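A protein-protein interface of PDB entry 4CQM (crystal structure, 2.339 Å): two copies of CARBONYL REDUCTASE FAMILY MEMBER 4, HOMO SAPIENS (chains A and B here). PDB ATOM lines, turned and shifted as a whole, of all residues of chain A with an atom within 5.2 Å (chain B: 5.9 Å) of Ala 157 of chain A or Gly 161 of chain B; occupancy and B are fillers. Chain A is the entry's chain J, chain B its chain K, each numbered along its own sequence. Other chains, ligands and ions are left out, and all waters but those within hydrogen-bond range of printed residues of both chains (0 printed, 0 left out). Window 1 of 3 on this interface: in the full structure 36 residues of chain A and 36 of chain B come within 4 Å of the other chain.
O of Gly 160 of chain A sits close to O of Gly 160 of chain B (3.4 Å).
CD2 of Leu 111 of chain A touches CD2 of Leu 115 of chain B, 3.99 Å away.
CD2 of Leu 115 of chain A touches CD2 of Leu 115 of chain B, 3.8 Å away.
Ser 153 of chain A touches Phe 165 of chain B (OG to CD1, 3.1 Å).
CB of Ser 156 of chain A touches O of Gly 164 of chain B (3.3 Å).
SD of Met 119 of chain B touches CB of Ala 157 of chain A, 3.8 Å away.
Phe 165 of chain B touches Ala 157 of chain A (CB to CB, 3.7 Å).
Gly 160 of chain A touches Gly 161 of chain B.
Ala 157 of chain B touches Gly 161 of chain A.
Gly 160 of chain B touches Gly 161 of chain A.
Gly 161 of chain A touches Gly 161 of chain B.
Of chain B, only Met 119 (3.8 Å), Gly 161 (3.2 Å) and Phe 165 (3.7 Å) come within 4 Å of Ala 157 of chain A.
Of the printed residues of chain A, Leu 115 of chain B touches Leu 111 (3.99 Å) and Leu 115 (3.8 Å).
Gly 161 of chain B touches just these residues of chain A: Ala 157 (3.2 Å), Gly 160 (3.9 Å) and Gly 161 (3.4 Å).
Of the printed residues of chain A, Phe 165 of chain B touches Ser 153 (3.1 Å) and Ala 157 (3.7 Å).
The nearest residue of chain B that does not touch Ala 157 of chain A is Leu 115 of chain B (4.1 Å).
The nearest residue of chain A that does not touch Gly 161 of chain B is Ser 156 of chain A (4.1 Å).
The nearest printed residue of chain B that does not touch Leu 115 of chain A is Ala 157 of chain B (4.4 Å).
Of the 14 printed residues of chain B, 7 touch a printed residue of chain A.
Printed residues of chain B that touch a printed residue of chain A: Leu 115, Met 119, Ala 157, Gly 160, Gly 161, Gly 164 and Phe 165.
Of the 12 printed residues of chain A, 7 touch a printed residue of chain B.
Hydrophobic or aromatic side chains of chain A that line the printed part of chain B: Leu 111, Leu 115 and Ala 157.
Among the printed residues, 13 pairs touch across the chains.
Ala 157 of chain A touches Gly 161 of chain B, and with the chains exchanged Gly 161 of chain A touches Ala 157 of chain B.
Gly 160 of chain A touches its own counterpart, Gly 160 of chain B.
Gly 160 of chain A touches Gly 161 of chain B, and with the chains exchanged Gly 161 of chain A touches Gly 160 of chain B.
Gly 161 of chain A touches its own counterpart, Gly 161 of chain B.
Positions printed for both chains: 115, 156, 157, 158, 159, 160 and 161.
Of the 13 pairs that touch across the chains among the printed residues, 7 have their exchanged pair printed and touching as well.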
ATOM      1  N   LEU A 111      10.877 -24.834  32.946  1.00  0.00           N
ATOM      2  CA  LEU A 111      11.006 -25.202  31.540  1.00  0.00           C
ATOM      3  C   LEU A 111      10.813 -26.700  31.326  1.00  0.00           C
ATOM      4  O   LEU A 111      10.243 -27.123  30.322  1.00  0.00           O
ATOM      5  CB  LEU A 111      12.370 -24.771  30.993  1.00  0.00           C
ATOM      6  CG  LEU A 111      12.422 -23.463  30.199  1.00  0.00           C
ATOM      7  CD1 LEU A 111      12.021 -22.276  31.059  1.00  0.00           C
ATOM      8  CD2 LEU A 111      13.806 -23.257  29.602  1.00  0.00           C
ATOM      9  N   LEU A 115       6.955 -27.148  30.042  1.00  0.00           N
ATOM     10  CA  LEU A 115       7.176 -27.215  28.602  1.00  0.00           C
ATOM     11  C   LEU A 115       7.699 -28.579  28.155  1.00  0.00           C
ATOM     12  O   LEU A 115       7.044 -29.280  27.383  1.00  0.00           O
ATOM     13  CB  LEU A 115       8.140 -26.110  28.168  1.00  0.00           C
ATOM     14  CG  LEU A 115       8.326 -25.903  26.665  1.00  0.00           C
ATOM     15  CD1 LEU A 115       6.978 -25.785  25.971  1.00  0.00           C
ATOM     16  CD2 LEU A 115       9.179 -24.671  26.396  1.00  0.00           C
ATOM     17  N   GLN A 152       6.384 -12.799  35.738  1.00  0.00           N
ATOM     18  CA  GLN A 152       6.137 -14.154  35.259  1.00  0.00           C
ATOM     19  C   GLN A 152       6.924 -14.426  33.982  1.00  0.00           C
ATOM     20  O   GLN A 152       6.374 -14.908  32.993  1.00  0.00           O
ATOM     21  CB  GLN A 152       4.643 -14.375  35.019  1.00  0.00           C
ATOM     22  CG  GLN A 152       3.800 -14.327  36.281  1.00  0.00           C
ATOM     23  CD  GLN A 152       2.332 -14.600  36.015  1.00  0.00           C
ATOM     24  OE1 GLN A 152       1.737 -14.027  35.101  1.00  0.00           O
ATOM     25  NE2 GLN A 152       1.740 -15.483  36.811  1.00  0.00           N
ATOM     26  N   SER A 153       8.216 -14.118  34.019  1.00  0.00           N
ATOM     27  CA  SER A 153       9.080 -14.241  32.849  1.00  0.00           C
ATOM     28  C   SER A 153       9.310 -15.695  32.444  1.00  0.00           C
ATOM     29  O   SER A 153       9.047 -16.077  31.304  1.00  0.00           O
ATOM     30  CB  SER A 153      10.422 -13.556  33.114  1.00  0.00           C
ATOM     31  OG  SER A 153      11.252 -13.596  31.968  1.00  0.00           O
ATOM     32  N   VAL A 154       9.805 -16.496  33.382  1.00  0.00           N
ATOM     33  CA  VAL A 154      10.095 -17.903  33.120  1.00  0.00           C
ATOM     34  C   VAL A 154       8.822 -18.675  32.788  1.00  0.00           C
ATOM     35  O   VAL A 154       8.819 -19.551  31.920  1.00  0.00           O
ATOM     36  CB  VAL A 154      10.793 -18.565  34.325  1.00  0.00           C
ATOM     37  CG1 VAL A 154      11.202 -19.990  33.988  1.00  0.00           C
ATOM     38  CG2 VAL A 154      12.004 -17.749  34.750  1.00  0.00           C
ATOM     39  N   TYR A 155       7.740 -18.338  33.482  1.00  0.00           N
ATOM     40  CA  TYR A 155       6.446 -18.971  33.259  1.00  0.00           C
ATOM     41  C   TYR A 155       5.924 -18.668  31.857  1.00  0.00           C
ATOM     42  O   TYR A 155       5.375 -19.542  31.187  1.00  0.00           O
ATOM     43  CB  TYR A 155       5.440 -18.509  34.314  1.00  0.00           C
ATOM     44  CG  TYR A 155       4.093 -19.187  34.223  1.00  0.00           C
ATOM     45  CD1 TYR A 155       3.924 -20.500  34.641  1.00  0.00           C
ATOM     46  CD2 TYR A 155       2.985 -18.509  33.729  1.00  0.00           C
ATOM     47  CE1 TYR A 155       2.693 -21.121  34.564  1.00  0.00           C
ATOM     48  CE2 TYR A 155       1.750 -19.123  33.647  1.00  0.00           C
ATOM     49  CZ  TYR A 155       1.611 -20.429  34.066  1.00  0.00           C
ATOM     50  OH  TYR A 155       0.384 -21.043  33.986  1.00  0.00           O
ATOM     51  N   SER A 156       6.102 -17.425  31.421  1.00  0.00           N
ATOM     52  CA  SER A 156       5.678 -17.013  30.089  1.00  0.00           C
ATOM     53  C   SER A 156       6.463 -17.762  29.019  1.00  0.00           C
ATOM     54  O   SER A 156       5.906 -18.177  28.002  1.00  0.00           O
ATOM     55  CB  SER A 156       5.853 -15.505  29.910  1.00  0.00           C
ATOM     56  OG  SER A 156       5.175 -14.790  30.927  1.00  0.00           O
ATOM     57  N   ALA A 157       7.759 -17.929  29.259  1.00  0.00           N
ATOM     58  CA  ALA A 157       8.626 -18.650  28.337  1.00  0.00           C
ATOM     59  C   ALA A 157       8.181 -20.102  28.191  1.00  0.00           C
ATOM     60  O   ALA A 157       8.014 -20.599  27.079  1.00  0.00           O
ATOM     61  CB  ALA A 157      10.070 -18.584  28.806  1.00  0.00           C
ATOM     62  N   SER A 158       7.987 -20.771  29.322  1.00  0.00           N
ATOM     63  CA  SER A 158       7.569 -22.168  29.325  1.00  0.00           C
ATOM     64  C   SER A 158       6.191 -22.344  28.693  1.00  0.00           C
ATOM     65  O   SER A 158       5.968 -23.277  27.922  1.00  0.00           O
ATOM     66  CB  SER A 158       7.570 -22.720  30.752  1.00  0.00           C
ATOM     67  OG  SER A 158       6.762 -21.930  31.606  1.00  0.00           O
ATOM     68  N   LYS A 159       5.270 -21.441  29.017  1.00  0.00           N
ATOM     69  CA  LYS A 159       3.919 -21.500  28.470  1.00  0.00           C
ATOM     70  C   LYS A 159       3.878 -21.024  27.023  1.00  0.00           C
ATOM     71  O   LYS A 159       2.980 -21.391  26.265  1.00  0.00           O
ATOM     72  CB  LYS A 159       2.958 -20.666  29.319  1.00  0.00           C
ATOM     73  CG  LYS A 159       2.683 -21.260  30.684  1.00  0.00           C
ATOM     74  CD  LYS A 159       2.072 -22.641  30.554  1.00  0.00           C
ATOM     75  CE  LYS A 159       2.045 -23.351  31.889  1.00  0.00           C
ATOM     76  NZ  LYS A 159       1.308 -24.643  31.817  1.00  0.00           N
ATOM     77  N   GLY A 160       4.854 -20.204  26.647  1.00  0.00           N
ATOM     78  CA  GLY A 160       4.921 -19.669  25.301  1.00  0.00           C
ATOM     79  C   GLY A 160       5.239 -20.735  24.273  1.00  0.00           C
ATOM     80  O   GLY A 160       4.612 -20.799  23.215  1.00  0.00           O
ATOM     81  N   GLY A 161       6.215 -21.579  24.589  1.00  0.00           N
ATOM     82  CA  GLY A 161       6.627 -22.638  23.688  1.00  0.00           C
ATOM     83  C   GLY A 161       5.570 -23.711  23.524  1.00  0.00           C
ATOM     84  O   GLY A 161       5.597 -24.479  22.564  1.00  0.00           O
ATOM     85  N   LEU B 115      16.140 -21.277  23.884  1.00  0.00           N
ATOM     86  CA  LEU B 115      15.223 -20.623  24.813  1.00  0.00           C
ATOM     87  C   LEU B 115      15.915 -20.190  26.104  1.00  0.00           C
ATOM     88  O   LEU B 115      16.018 -18.996  26.386  1.00  0.00           O
ATOM     89  CB  LEU B 115      14.045 -21.544  25.136  1.00  0.00           C
ATOM     90  CG  LEU B 115      13.018 -21.015  26.139  1.00  0.00           C
ATOM     91  CD1 LEU B 115      12.471 -19.674  25.688  1.00  0.00           C
ATOM     92  CD2 LEU B 115      11.892 -22.018  26.331  1.00  0.00           C
ATOM     93  N   MET B 119      17.433 -16.498  27.743  1.00  0.00           N
ATOM     94  CA  MET B 119      16.989 -16.014  29.046  1.00  0.00           C
ATOM     95  C   MET B 119      18.182 -15.664  29.927  1.00  0.00           C
ATOM     96  O   MET B 119      18.135 -14.707  30.699  1.00  0.00           O
ATOM     97  CB  MET B 119      16.109 -17.053  29.745  1.00  0.00           C
ATOM     98  CG  MET B 119      14.875 -17.456  28.958  1.00  0.00           C
ATOM     99  SD  MET B 119      13.655 -18.322  29.966  1.00  0.00           S
ATOM    100  CE  MET B 119      14.677 -19.552  30.764  1.00  0.00           C
ATOM    101  N   GLY B 145       7.801 -20.616  15.251  1.00  0.00           N
ATOM    102  CA  GLY B 145       7.677 -20.518  16.692  1.00  0.00           C
ATOM    103  C   GLY B 145       6.266 -20.131  17.088  1.00  0.00           C
ATOM    104  O   GLY B 145       5.825 -20.403  18.204  1.00  0.00           O
ATOM    105  N   SER B 156      10.086 -25.372  17.266  1.00  0.00           N
ATOM    106  CA  SER B 156       8.950 -24.467  17.398  1.00  0.00           C
ATOM    107  C   SER B 156       8.708 -24.077  18.852  1.00  0.00           C
ATOM    108  O   SER B 156       8.424 -22.918  19.155  1.00  0.00           O
ATOM    109  CB  SER B 156       7.690 -25.104  16.813  1.00  0.00           C
ATOM    110  OG  SER B 156       7.890 -25.479  15.462  1.00  0.00           O
ATOM    111  N   ALA B 157       8.817 -25.053  19.748  1.00  0.00           N
ATOM    112  CA  ALA B 157       8.649 -24.803  21.174  1.00  0.00           C
ATOM    113  C   ALA B 157       9.722 -23.849  21.681  1.00  0.00           C
ATOM    114  O   ALA B 157       9.431 -22.879  22.379  1.00  0.00           O
ATOM    115  CB  ALA B 157       8.691 -26.107  21.951  1.00  0.00           C
ATOM    116  N   SER B 158      10.968 -24.129  21.315  1.00  0.00           N
ATOM    117  CA  SER B 158      12.095 -23.311  21.739  1.00  0.00           C
ATOM    118  C   SER B 158      12.015 -21.900  21.161  1.00  0.00           C
ATOM    119  O   SER B 158      12.434 -20.936  21.802  1.00  0.00           O
ATOM    120  CB  SER B 158      13.412 -23.972  21.333  1.00  0.00           C
ATOM    121  OG  SER B 158      13.472 -24.167  19.930  1.00  0.00           O
ATOM    122  N   LYS B 159      11.472 -21.782  19.954  1.00  0.00           N
ATOM    123  CA  LYS B 159      11.364 -20.484  19.293  1.00  0.00           C
ATOM    124  C   LYS B 159      10.040 -19.794  19.597  1.00  0.00           C
ATOM    125  O   LYS B 159       9.862 -18.615  19.294  1.00  0.00           O
ATOM    126  CB  LYS B 159      11.540 -20.635  17.782  1.00  0.00           C
ATOM    127  CG  LYS B 159      12.965 -20.948  17.375  1.00  0.00           C
ATOM    128  CD  LYS B 159      13.927 -19.957  18.010  1.00  0.00           C
ATOM    129  CE  LYS B 159      15.364 -20.409  17.856  1.00  0.00           C
ATOM    130  NZ  LYS B 159      16.310 -19.503  18.566  1.00  0.00           N
ATOM    131  N   GLY B 160       9.113 -20.532  20.195  1.00  0.00           N
ATOM    132  CA  GLY B 160       7.843 -19.961  20.597  1.00  0.00           C
ATOM    133  C   GLY B 160       7.900 -19.486  22.033  1.00  0.00           C
ATOM    134  O   GLY B 160       7.124 -18.625  22.449  1.00  0.00           O
ATOM    135  N   GLY B 161       8.835 -20.052  22.790  1.00  0.00           N
ATOM    136  CA  GLY B 161       8.984 -19.730  24.194  1.00  0.00           C
ATOM    137  C   GLY B 161       9.484 -18.322  24.452  1.00  0.00           C
ATOM    138  O   GLY B 161       8.955 -17.618  25.311  1.00  0.00           O
ATOM    139  N   LEU B 162      10.499 -17.903  23.702  1.00  0.00           N
ATOM    140  CA  LEU B 162      11.121 -16.602  23.933  1.00  0.00           C
ATOM    141  C   LEU B 162      10.307 -15.469  23.312  1.00  0.00           C
ATOM    142  O   LEU B 162      10.762 -14.327  23.255  1.00  0.00           O
ATOM    143  CB  LEU B 162      12.559 -16.583  23.400  1.00  0.00           C
ATOM    144  CG  LEU B 162      12.850 -16.362  21.912  1.00  0.00           C
ATOM    145  CD1 LEU B 162      14.347 -16.218  21.693  1.00  0.00           C
ATOM    146  CD2 LEU B 162      12.301 -17.488  21.063  1.00  0.00           C
ATOM    147  N   VAL B 163       9.103 -15.789  22.853  1.00  0.00           N
ATOM    148  CA  VAL B 163       8.158 -14.770  22.423  1.00  0.00           C
ATOM    149  C   VAL B 163       7.398 -14.257  23.641  1.00  0.00           C
ATOM    150  O   VAL B 163       7.262 -13.050  23.842  1.00  0.00           O
ATOM    151  CB  VAL B 163       7.166 -15.306  21.374  1.00  0.00           C
ATOM    152  CG1 VAL B 163       6.093 -14.270  21.073  1.00  0.00           C
ATOM    153  CG2 VAL B 163       7.903 -15.704  20.104  1.00  0.00           C
ATOM    154  N   GLY B 164       6.912 -15.187  24.457  1.00  0.00           N
ATOM    155  CA  GLY B 164       6.250 -14.841  25.700  1.00  0.00           C
ATOM    156  C   GLY B 164       7.248 -14.326  26.718  1.00  0.00           C
ATOM    157  O   GLY B 164       6.924 -13.471  27.542  1.00  0.00           O
ATOM    158  N   PHE B 165       8.468 -14.848  26.653  1.00  0.00           N
ATOM    159  CA  PHE B 165       9.547 -14.409  27.533  1.00  0.00           C
ATOM    160  C   PHE B 165       9.919 -12.955  27.277  1.00  0.00           C
ATOM    161  O   PHE B 165       9.985 -12.149  28.206  1.00  0.00           O
ATOM    162  CB  PHE B 165      10.780 -15.298  27.354  1.00  0.00           C
ATOM    163  CG  PHE B 165      12.048 -14.692  27.889  1.00  0.00           C
ATOM    164  CD1 PHE B 165      12.314 -14.694  29.248  1.00  0.00           C
ATOM    165  CD2 PHE B 165      12.978 -14.123  27.031  1.00  0.00           C
ATOM    166  CE1 PHE B 165      13.477 -14.137  29.743  1.00  0.00           C
ATOM    167  CE2 PHE B 165      14.144 -13.564  27.521  1.00  0.00           C
ATOM    168  CZ  PHE B 165      14.394 -13.571  28.878  1.00  0.00           C
ATOM    169  N   SER B 166      10.172 -12.634  26.011  1.00  0.00           N
ATOM    170  CA  SER B 166      10.565 -11.287  25.615  1.00  0.00           C
ATOM    171  C   SER B 166       9.494 -10.277  25.987  1.00  0.00           C
ATOM    172  O   SER B 166       9.795  -9.160  26.411  1.00  0.00           O
ATOM    173  CB  SER B 166      10.838 -11.224  24.114  1.00  0.00           C
ATOM    174  OG  SER B 166      11.877 -12.111  23.746  1.00  0.00           O
